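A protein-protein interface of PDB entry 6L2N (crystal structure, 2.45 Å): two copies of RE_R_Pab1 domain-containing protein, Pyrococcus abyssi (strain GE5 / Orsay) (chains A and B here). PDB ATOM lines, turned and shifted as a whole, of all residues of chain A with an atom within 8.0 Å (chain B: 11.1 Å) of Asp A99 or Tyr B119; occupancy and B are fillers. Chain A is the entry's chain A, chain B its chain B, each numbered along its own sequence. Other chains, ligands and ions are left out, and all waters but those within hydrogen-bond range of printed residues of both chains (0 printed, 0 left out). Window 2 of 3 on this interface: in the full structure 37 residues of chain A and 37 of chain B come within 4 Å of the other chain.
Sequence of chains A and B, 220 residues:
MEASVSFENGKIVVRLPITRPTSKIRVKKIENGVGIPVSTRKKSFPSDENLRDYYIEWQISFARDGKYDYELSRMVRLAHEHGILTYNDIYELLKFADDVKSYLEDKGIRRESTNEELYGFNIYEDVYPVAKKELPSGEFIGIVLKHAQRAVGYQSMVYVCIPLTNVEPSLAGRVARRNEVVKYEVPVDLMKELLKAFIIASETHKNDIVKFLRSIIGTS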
ATOM      1  N   GLU A  92       0.260  13.965  12.790  1.00  0.00           N
ATOM      2  CA  GLU A  92       0.461  15.147  13.617  1.00  0.00           C
ATOM      3  C   GLU A  92       1.813  15.802  13.378  1.00  0.00           C
ATOM      4  O   GLU A  92       1.960  17.001  13.641  1.00  0.00           O
ATOM      5  CB  GLU A  92       0.299  14.794  15.100  1.00  0.00           C
ATOM      6  CG  GLU A  92       1.497  14.117  15.742  1.00  0.00           C
ATOM      7  CD  GLU A  92       1.621  14.458  17.215  1.00  0.00           C
ATOM      8  OE1 GLU A  92       2.683  14.180  17.807  1.00  0.00           O
ATOM      9  OE2 GLU A  92       0.654  15.013  17.777  1.00  0.00           O
ATOM     10  N   LEU A  93       2.803  15.049  12.891  1.00  0.00           N
ATOM     11  CA  LEU A  93       4.042  15.673  12.440  1.00  0.00           C
ATOM     12  C   LEU A  93       3.779  16.599  11.261  1.00  0.00           C
ATOM     13  O   LEU A  93       4.356  17.690  11.175  1.00  0.00           O
ATOM     14  CB  LEU A  93       5.069  14.604  12.066  1.00  0.00           C
ATOM     15  CG  LEU A  93       5.908  14.003  13.197  1.00  0.00           C
ATOM     16  CD1 LEU A  93       6.616  12.740  12.731  1.00  0.00           C
ATOM     17  CD2 LEU A  93       6.911  15.017  13.726  1.00  0.00           C
ATOM     18  N   LEU A  94       2.901  16.183  10.346  1.00  0.00           N
ATOM     19  CA  LEU A  94       2.528  17.038   9.224  1.00  0.00           C
ATOM     20  C   LEU A  94       1.737  18.254   9.687  1.00  0.00           C
ATOM     21  O   LEU A  94       1.872  19.337   9.104  1.00  0.00           O
ATOM     22  CB  LEU A  94       1.722  16.237   8.202  1.00  0.00           C
ATOM     23  CG  LEU A  94       2.517  15.267   7.327  1.00  0.00           C
ATOM     24  CD1 LEU A  94       1.625  14.140   6.826  1.00  0.00           C
ATOM     25  CD2 LEU A  94       3.164  16.002   6.165  1.00  0.00           C
ATOM     26  N   LYS A  95       0.908  18.099  10.722  1.00  0.00           N
ATOM     27  CA  LYS A  95       0.186  19.244  11.264  1.00  0.00           C
ATOM     28  C   LYS A  95       1.132  20.223  11.945  1.00  0.00           C
ATOM     29  O   LYS A  95       0.900  21.436  11.907  1.00  0.00           O
ATOM     30  CB  LYS A  95      -0.893  18.775  12.240  1.00  0.00           C
ATOM     31  CG  LYS A  95      -2.298  18.799  11.660  1.00  0.00           C
ATOM     32  CD  LYS A  95      -2.350  18.076  10.325  1.00  0.00           C
ATOM     33  CE  LYS A  95      -3.619  18.406   9.560  1.00  0.00           C
ATOM     34  NZ  LYS A  95      -3.593  17.826   8.189  1.00  0.00           N
ATOM     35  N   PHE A  96       2.197  19.716  12.571  1.00  0.00           N
ATOM     36  CA  PHE A  96       3.227  20.596  13.109  1.00  0.00           C
ATOM     37  C   PHE A  96       3.967  21.327  11.997  1.00  0.00           C
ATOM     38  O   PHE A  96       4.361  22.486  12.174  1.00  0.00           O
ATOM     39  CB  PHE A  96       4.205  19.790  13.968  1.00  0.00           C
ATOM     40  CG  PHE A  96       5.402  20.575  14.434  1.00  0.00           C
ATOM     41  CD1 PHE A  96       5.326  21.374  15.563  1.00  0.00           C
ATOM     42  CD2 PHE A  96       6.605  20.505  13.749  1.00  0.00           C
ATOM     43  CE1 PHE A  96       6.425  22.095  15.996  1.00  0.00           C
ATOM     44  CE2 PHE A  96       7.707  21.223  14.177  1.00  0.00           C
ATOM     45  CZ  PHE A  96       7.617  22.018  15.302  1.00  0.00           C
ATOM     46  N   ALA A  97       4.158  20.674  10.848  1.00  0.00           N
ATOM     47  CA  ALA A  97       4.835  21.323   9.730  1.00  0.00           C
ATOM     48  C   ALA A  97       3.958  22.387   9.084  1.00  0.00           C
ATOM     49  O   ALA A  97       4.473  23.402   8.598  1.00  0.00           O
ATOM     50  CB  ALA A  97       5.252  20.282   8.691  1.00  0.00           C
ATOM     51  N   ASP A  98       2.640  22.176   9.061  1.00  0.00           N
ATOM     52  CA  ASP A  98       1.743  23.178   8.499  1.00  0.00           C
ATOM     53  C   ASP A  98       1.722  24.446   9.344  1.00  0.00           C
ATOM     54  O   ASP A  98       1.589  25.550   8.801  1.00  0.00           O
ATOM     55  CB  ASP A  98       0.331  22.605   8.369  1.00  0.00           C
ATOM     56  CG  ASP A  98      -0.476  23.292   7.284  1.00  0.00           C
ATOM     57  OD1 ASP A  98      -0.001  23.337   6.130  1.00  0.00           O
ATOM     58  OD2 ASP A  98      -1.583  23.787   7.585  1.00  0.00           O
ATOM     59  N   ASP A  99       1.865  24.314  10.665  1.00  0.00           N
ATOM     60  CA  ASP A  99       1.811  25.468  11.553  1.00  0.00           C
ATOM     61  C   ASP A  99       3.125  26.238  11.614  1.00  0.00           C
ATOM     62  O   ASP A  99       3.120  27.404  12.023  1.00  0.00           O
ATOM     63  CB  ASP A  99       1.424  25.037  12.967  1.00  0.00           C
ATOM     64  CG  ASP A  99       0.119  24.269  13.010  1.00  0.00           C
ATOM     65  OD1 ASP A  99      -0.101  23.524  13.987  1.00  0.00           O
ATOM     66  OD2 ASP A  99      -0.691  24.413  12.071  1.00  0.00           O
ATOM     67  N   VAL A 100       4.244  25.624  11.230  1.00  0.00           N
ATOM     68  CA  VAL A 100       5.534  26.296  11.340  1.00  0.00           C
ATOM     69  C   VAL A 100       5.616  27.381  10.272  1.00  0.00           C
ATOM     70  O   VAL A 100       5.483  27.105   9.074  1.00  0.00           O
ATOM     71  CB  VAL A 100       6.688  25.289  11.228  1.00  0.00           C
ATOM     72  CG1 VAL A 100       7.942  25.955  10.671  1.00  0.00           C
ATOM     73  CG2 VAL A 100       6.972  24.664  12.588  1.00  0.00           C
ATOM     74  N   LYS A 101       5.814  28.629  10.707  1.00  0.00           N
ATOM     75  CA  LYS A 101       5.829  29.774   9.806  1.00  0.00           C
ATOM     76  C   LYS A 101       7.163  30.507   9.769  1.00  0.00           C
ATOM     77  O   LYS A 101       7.390  31.292   8.842  1.00  0.00           O
ATOM     78  CB  LYS A 101       4.729  30.773  10.195  1.00  0.00           C
ATOM     79  CG  LYS A 101       3.343  30.142  10.306  1.00  0.00           C
ATOM     80  CD  LYS A 101       2.393  30.987  11.145  1.00  0.00           C
ATOM     81  CE  LYS A 101       1.519  30.112  12.033  1.00  0.00           C
ATOM     82  NZ  LYS A 101       0.087  30.522  12.010  1.00  0.00           N
ATOM     83  N   SER A 102       8.044  30.282  10.744  1.00  0.00           N
ATOM     84  CA  SER A 102       9.382  30.857  10.759  1.00  0.00           C
ATOM     85  C   SER A 102      10.398  29.742  10.957  1.00  0.00           C
ATOM     86  O   SER A 102      10.086  28.687  11.520  1.00  0.00           O
ATOM     87  CB  SER A 102       9.532  31.914  11.859  1.00  0.00           C
ATOM     88  OG  SER A 102       9.061  31.425  13.103  1.00  0.00           O
ATOM     89  N   TYR A 103      11.619  29.985  10.489  1.00  0.00           N
ATOM     90  CA  TYR A 103      12.653  28.964  10.451  1.00  0.00           C
ATOM     91  C   TYR A 103      13.976  29.533  10.942  1.00  0.00           C
ATOM     92  O   TYR A 103      14.181  30.749  10.983  1.00  0.00           O
ATOM     93  CB  TYR A 103      12.833  28.384   9.032  1.00  0.00           C
ATOM     94  CG  TYR A 103      11.538  27.987   8.350  1.00  0.00           C
ATOM     95  CD1 TYR A 103      11.181  26.651   8.223  1.00  0.00           C
ATOM     96  CD2 TYR A 103      10.690  28.946   7.806  1.00  0.00           C
ATOM     97  CE1 TYR A 103      10.000  26.283   7.595  1.00  0.00           C
ATOM     98  CE2 TYR A 103       9.510  28.589   7.184  1.00  0.00           C
ATOM     99  CZ  TYR A 103       9.171  27.260   7.077  1.00  0.00           C
ATOM    100  OH  TYR A 103       7.994  26.922   6.448  1.00  0.00           O
ATOM    101  N   LEU A 104      14.877  28.622  11.324  1.00  0.00           N
ATOM    102  CA  LEU A 104      16.221  29.016  11.737  1.00  0.00           C
ATOM    103  C   LEU A 104      16.935  29.784  10.633  1.00  0.00           C
ATOM    104  O   LEU A 104      17.710  30.704  10.915  1.00  0.00           O
ATOM    105  CB  LEU A 104      17.016  27.769  12.139  1.00  0.00           C
ATOM    106  CG  LEU A 104      18.394  27.877  12.801  1.00  0.00           C
ATOM    107  CD1 LEU A 104      19.508  27.874  11.764  1.00  0.00           C
ATOM    108  CD2 LEU A 104      18.485  29.104  13.698  1.00  0.00           C
ATOM    109  N   LYS A 133      18.368  21.743  21.421  1.00  0.00           N
ATOM    110  CA  LYS A 133      17.288  21.131  22.186  1.00  0.00           C
ATOM    111  C   LYS A 133      17.809  19.872  22.861  1.00  0.00           C
ATOM    112  O   LYS A 133      18.450  19.039  22.214  1.00  0.00           O
ATOM    113  CB  LYS A 133      16.090  20.791  21.292  1.00  0.00           C
ATOM    114  CG  LYS A 133      14.939  20.117  22.029  1.00  0.00           C
ATOM    115  CD  LYS A 133      13.743  19.905  21.115  1.00  0.00           C
ATOM    116  CE  LYS A 133      12.432  20.026  21.877  1.00  0.00           C
ATOM    117  NZ  LYS A 133      11.284  20.278  20.962  1.00  0.00           N
ATOM    118  N   GLU A 193      11.694  14.354  16.999  1.00  0.00           N
ATOM    119  CA  GLU A 193      12.368  15.631  17.218  1.00  0.00           C
ATOM    120  C   GLU A 193      13.388  15.922  16.127  1.00  0.00           C
ATOM    121  O   GLU A 193      13.664  17.091  15.832  1.00  0.00           O
ATOM    122  CB  GLU A 193      13.039  15.640  18.592  1.00  0.00           C
ATOM    123  CG  GLU A 193      12.077  15.463  19.758  1.00  0.00           C
ATOM    124  CD  GLU A 193      11.195  16.677  19.980  1.00  0.00           C
ATOM    125  OE1 GLU A 193      11.571  17.781  19.531  1.00  0.00           O
ATOM    126  OE2 GLU A 193      10.125  16.529  20.607  1.00  0.00           O
ATOM    127  N   LYS A 196      11.231  17.093  13.264  1.00  0.00           N
ATOM    128  CA  LYS A 196      10.826  18.462  13.562  1.00  0.00           C
ATOM    129  C   LYS A 196      11.984  19.435  13.367  1.00  0.00           C
ATOM    130  O   LYS A 196      11.781  20.561  12.901  1.00  0.00           O
ATOM    131  CB  LYS A 196      10.286  18.551  14.989  1.00  0.00           C
ATOM    132  CG  LYS A 196       8.959  17.839  15.193  1.00  0.00           C
ATOM    133  CD  LYS A 196       8.688  17.578  16.666  1.00  0.00           C
ATOM    134  CE  LYS A 196       8.670  18.869  17.466  1.00  0.00           C
ATOM    135  NZ  LYS A 196       8.411  18.623  18.911  1.00  0.00           N
ATOM    136  N   ALA A 197      13.204  19.016  13.717  1.00  0.00           N
ATOM    137  CA  ALA A 197      14.367  19.881  13.537  1.00  0.00           C
ATOM    138  C   ALA A 197      14.527  20.283  12.077  1.00  0.00           C
ATOM    139  O   ALA A 197      14.723  21.461  11.762  1.00  0.00           O
ATOM    140  CB  ALA A 197      15.628  19.180  14.047  1.00  0.00           C
ATOM    141  N   ILE A 199      12.175  20.381  10.004  1.00  0.00           N
ATOM    142  CA  ILE A 199      11.003  21.168   9.635  1.00  0.00           C
ATOM    143  C   ILE A 199      11.235  22.648   9.929  1.00  0.00           C
ATOM    144  O   ILE A 199      10.844  23.520   9.142  1.00  0.00           O
ATOM    145  CB  ILE A 199       9.752  20.628  10.355  1.00  0.00           C
ATOM    146  CG1 ILE A 199       9.278  19.324   9.705  1.00  0.00           C
ATOM    147  CG2 ILE A 199       8.632  21.657  10.354  1.00  0.00           C
ATOM    148  CD1 ILE A 199       8.116  18.660  10.428  1.00  0.00           C
ATOM    149  N   ILE A 200      11.889  22.958  11.055  1.00  0.00           N
ATOM    150  CA  ILE A 200      12.117  24.349  11.439  1.00  0.00           C
ATOM    151  C   ILE A 200      13.460  24.893  10.970  1.00  0.00           C
ATOM    152  O   ILE A 200      13.733  26.087  11.166  1.00  0.00           O
ATOM    153  CB  ILE A 200      12.032  24.538  12.968  1.00  0.00           C
ATOM    154  CG1 ILE A 200      13.170  23.789  13.662  1.00  0.00           C
ATOM    155  CG2 ILE A 200      10.678  24.077  13.490  1.00  0.00           C
ATOM    156  CD1 ILE A 200      13.424  24.245  15.081  1.00  0.00           C
ATOM    157  N   ALA A 201      14.314  24.061  10.369  1.00  0.00           N
ATOM    158  CA  ALA A 201      15.609  24.547   9.902  1.00  0.00           C
ATOM    159  C   ALA A 201      15.442  25.538   8.755  1.00  0.00           C
ATOM    160  O   ALA A 201      15.945  26.666   8.816  1.00  0.00           O
ATOM    161  CB  ALA A 201      16.491  23.373   9.479  1.00  0.00           C
ATOM    162  N   LYS A 206      11.847  21.715   5.159  1.00  0.00           N
ATOM    163  CA  LYS A 206      10.511  21.317   5.596  1.00  0.00           C
ATOM    164  C   LYS A 206       9.731  20.659   4.464  1.00  0.00           C
ATOM    165  O   LYS A 206       9.108  19.607   4.654  1.00  0.00           O
ATOM    166  CB  LYS A 206       9.745  22.524   6.135  1.00  0.00           C
ATOM    167  CG  LYS A 206       8.336  22.181   6.596  1.00  0.00           C
ATOM    168  CD  LYS A 206       7.573  23.410   7.054  1.00  0.00           C
ATOM    169  CE  LYS A 206       6.825  24.065   5.904  1.00  0.00           C
ATOM    170  NZ  LYS A 206       6.109  25.292   6.355  1.00  0.00           N
ATOM    171  N   THR B 114      20.223  33.973  23.244  1.00  0.00           N
ATOM    172  CA  THR B 114      19.070  34.842  23.087  1.00  0.00           C
ATOM    173  C   THR B 114      17.881  34.247  23.834  1.00  0.00           C
ATOM    174  O   THR B 114      17.828  33.047  24.112  1.00  0.00           O
ATOM    175  CB  THR B 114      18.720  35.035  21.609  1.00  0.00           C
ATOM    176  OG1 THR B 114      18.014  33.884  21.129  1.00  0.00           O
ATOM    177  CG2 THR B 114      19.983  35.227  20.782  1.00  0.00           C
ATOM    178  N   ASN B 115      16.925  35.108  24.170  1.00  0.00           N
ATOM    179  CA  ASN B 115      15.725  34.667  24.869  1.00  0.00           C
ATOM    180  C   ASN B 115      14.680  34.077  23.929  1.00  0.00           C
ATOM    181  O   ASN B 115      13.526  33.906  24.338  1.00  0.00           O
ATOM    182  CB  ASN B 115      15.123  35.830  25.662  1.00  0.00           C
ATOM    183  CG  ASN B 115      15.946  36.186  26.885  1.00  0.00           C
ATOM    184  OD1 ASN B 115      17.067  35.707  27.056  1.00  0.00           O
ATOM    185  ND2 ASN B 115      15.389  37.031  27.747  1.00  0.00           N
ATOM    186  N   GLU B 116      15.058  33.755  22.696  1.00  0.00           N
ATOM    187  CA  GLU B 116      14.128  33.238  21.706  1.00  0.00           C
ATOM    188  C   GLU B 116      14.044  31.717  21.780  1.00  0.00           C
ATOM    189  O   GLU B 116      15.005  31.035  22.143  1.00  0.00           O
ATOM    190  CB  GLU B 116      14.549  33.664  20.297  1.00  0.00           C
ATOM    191  CG  GLU B 116      14.323  35.137  19.994  1.00  0.00           C
ATOM    192  CD  GLU B 116      15.222  35.648  18.883  1.00  0.00           C
ATOM    193  OE1 GLU B 116      16.342  35.117  18.731  1.00  0.00           O
ATOM    194  OE2 GLU B 116      14.807  36.579  18.161  1.00  0.00           O
ATOM    195  N   GLU B 117      12.872  31.194  21.427  1.00  0.00           N
ATOM    196  CA  GLU B 117      12.633  29.759  21.347  1.00  0.00           C
ATOM    197  C   GLU B 117      11.901  29.473  20.046  1.00  0.00           C
ATOM    198  O   GLU B 117      10.809  30.004  19.817  1.00  0.00           O
ATOM    199  CB  GLU B 117      11.825  29.255  22.546  1.00  0.00           C
ATOM    200  CG  GLU B 117      12.626  29.143  23.832  1.00  0.00           C
ATOM    201  CD  GLU B 117      11.929  28.294  24.877  1.00  0.00           C
ATOM    202  OE1 GLU B 117      10.737  27.974  24.686  1.00  0.00           O
ATOM    203  OE2 GLU B 117      12.574  27.946  25.889  1.00  0.00           O
ATOM    204  N   LEU B 118      12.501  28.646  19.197  1.00  0.00           N
ATOM    205  CA  LEU B 118      11.952  28.338  17.878  1.00  0.00           C
ATOM    206  C   LEU B 118      11.271  26.974  17.948  1.00  0.00           C
ATOM    207  O   LEU B 118      11.894  25.935  17.732  1.00  0.00           O
ATOM    208  CB  LEU B 118      13.044  28.370  16.815  1.00  0.00           C
ATOM    209  CG  LEU B 118      12.563  28.168  15.378  1.00  0.00           C
ATOM    210  CD1 LEU B 118      11.574  29.252  14.981  1.00  0.00           C
ATOM    211  CD2 LEU B 118      13.738  28.126  14.418  1.00  0.00           C
ATOM    212  N   TYR B 119       9.973  26.992  18.256  1.00  0.00           N
ATOM    213  CA  TYR B 119       9.141  25.788  18.311  1.00  0.00           C
ATOM    214  C   TYR B 119       9.755  24.730  19.225  1.00  0.00           C
ATOM    215  O   TYR B 119       9.932  23.569  18.849  1.00  0.00           O
ATOM    216  CB  TYR B 119       8.898  25.231  16.907  1.00  0.00           C
ATOM    217  CG  TYR B 119       8.088  26.158  16.029  1.00  0.00           C
ATOM    218  CD1 TYR B 119       6.722  26.310  16.223  1.00  0.00           C
ATOM    219  CD2 TYR B 119       8.691  26.888  15.012  1.00  0.00           C
ATOM    220  CE1 TYR B 119       5.977  27.158  15.428  1.00  0.00           C
ATOM    221  CE2 TYR B 119       7.954  27.738  14.211  1.00  0.00           C
ATOM    222  CZ  TYR B 119       6.598  27.869  14.423  1.00  0.00           C
ATOM    223  OH  TYR B 119       5.858  28.713  13.629  1.00  0.00           O
ATOM    224  N   GLY B 120      10.082  25.147  20.447  1.00  0.00           N
ATOM    225  CA  GLY B 120      10.666  24.263  21.430  1.00  0.00           C
ATOM    226  C   GLY B 120      12.178  24.199  21.428  1.00  0.00           C
ATOM    227  O   GLY B 120      12.755  23.596  22.343  1.00  0.00           O
ATOM    228  N   PHE B 121      12.839  24.795  20.440  1.00  0.00           N
ATOM    229  CA  PHE B 121      14.294  24.787  20.350  1.00  0.00           C
ATOM    230  C   PHE B 121      14.842  26.108  20.873  1.00  0.00           C
ATOM    231  O   PHE B 121      14.348  27.178  20.505  1.00  0.00           O
ATOM    232  CB  PHE B 121      14.752  24.568  18.905  1.00  0.00           C
ATOM    233  CG  PHE B 121      14.603  23.150  18.423  1.00  0.00           C
ATOM    234  CD1 PHE B 121      13.348  22.608  18.192  1.00  0.00           C
ATOM    235  CD2 PHE B 121      15.719  22.364  18.185  1.00  0.00           C
ATOM    236  CE1 PHE B 121      13.209  21.307  17.742  1.00  0.00           C
ATOM    237  CE2 PHE B 121      15.587  21.060  17.736  1.00  0.00           C
ATOM    238  CZ  PHE B 121      14.331  20.533  17.514  1.00  0.00           C
ATOM    239  N   ASN B 122      15.864  26.032  21.722  1.00  0.00           N
ATOM    240  CA  ASN B 122      16.517  27.234  22.223  1.00  0.00           C
ATOM    241  C   ASN B 122      17.435  27.806  21.148  1.00  0.00           C
ATOM    242  O   ASN B 122      18.177  27.065  20.495  1.00  0.00           O
ATOM    243  CB  ASN B 122      17.309  26.928  23.492  1.00  0.00           C
ATOM    244  CG  ASN B 122      16.416  26.620  24.680  1.00  0.00           C
ATOM    245  OD1 ASN B 122      15.195  26.524  24.545  1.00  0.00           O
ATOM    246  ND2 ASN B 122      17.022  26.460  25.849  1.00  0.00           N
ATOM    247  N   ILE B 123      17.385  29.123  20.966  1.00  0.00           N
ATOM    248  CA  ILE B 123      18.133  29.810  19.920  1.00  0.00           C
ATOM    249  C   ILE B 123      19.296  30.556  20.559  1.00  0.00           C
ATOM    250  O   ILE B 123      19.111  31.291  21.536  1.00  0.00           O
ATOM    251  CB  ILE B 123      17.231  30.769  19.123  1.00  0.00           C
ATOM    252  CG1 ILE B 123      16.155  29.982  18.370  1.00  0.00           C
ATOM    253  CG2 ILE B 123      18.059  31.608  18.161  1.00  0.00           C
ATOM    254  CD1 ILE B 123      16.693  29.170  17.209  1.00  0.00           C
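No position is printed for both chains.
The side-chain carboxylate (OE2) of Glu A193 is in salt-bridge range of the side-chain amino group (NZ) of Lys A196 (3.2 Å).
N of Leu A104 sits at hydrogen-bond distance from O of Ala A201 (3.4 Å).
The backbone carbonyl oxygen (O) of Ile B123 lies within hydrogen-bond range of the side-chain hydroxyl (OG1) of Thr B114, 2.8 Å away.
NZ of Lys A206 is in hydrogen-bond range of O of Val A100, 3.3 Å away.
O of Glu B116 is in hydrogen-bond range of N of Ile B123.
The backbone carbonyl oxygen (O) of Ile A200 sits at hydrogen-bond distance from the backbone NH (N) of Leu A104 (2.8 Å).
Among the printed residues, merely in contact across the chains: Leu A104 with Leu B118, Val A100 with Tyr B119, Ile A200 with Leu B118, Lys A133 with Phe B121, Ile A200 with Phe B121, Ser A102 with Tyr B119, Lys A133 with Gly B120, Tyr A103 with Leu B118, Ile A200 with Tyr B119, Ser A102 with Leu B118, Phe A96 with Tyr B119, Glu A193 with Phe B121, Ala A197 with Phe B121 and Leu A104 with Ile B123.
Of chain B, only Tyr B119 comes within 4 Å of Asp A99.
Tyr B119 touches just these residues of chain A: Phe A96, Asp A99, Val A100, Lys A101, Ser A102 and Ile A200.
Of chain B, only Tyr B119 comes within 4 Å of Phe A96.
No residue of chain B comes within 4 Å of Asp A98.
Of chain B, only Tyr B119 comes within 4 Å of Lys A101.
Ser A102 touches just these residues of chain B: Leu B118 (3.8 Å) and Tyr B119 (3.6 Å).
Of the printed residues of chain A, Phe B121 touches Lys A133 (3.5 Å), Glu A193 (3.9 Å), Ala A197 (3.9 Å) and Ile A200 (3.5 Å).
Printed residues of chain A within 4 Å of Leu B118: Ser A102 (3.8 Å), Tyr A103 (3.8 Å), Leu A104 (3.3 Å) and Ile A200 (3.5 Å).
Glu B116 touches none of the printed residues of chain A.
Glu B117 touches none of the printed residues of chain A.
The nearest residue of chain B that does not touch Asp A99 is Leu B118 (9.1 Å).
The nearest printed residue of chain B that does not touch Lys A133 is Tyr B119 (4.1 Å).
N of Lys A101 sits at hydrogen-bond distance from OH of Tyr B119, at 2.9 Å.
The side-chain hydroxyl of Tyr B119 lies within hydrogen-bond range of the backbone carbonyl oxygen of Asp A99, 3.4 Å away.
Of the 10 printed residues of chain B, 5 touch a printed residue of chain A.
Hydrophobic or aromatic side chains of chain B that line the printed part of chain A: Leu B118, Tyr B119, Phe B121 and Ile B123.
Among the printed residues, 16 pairs touch across the chains.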
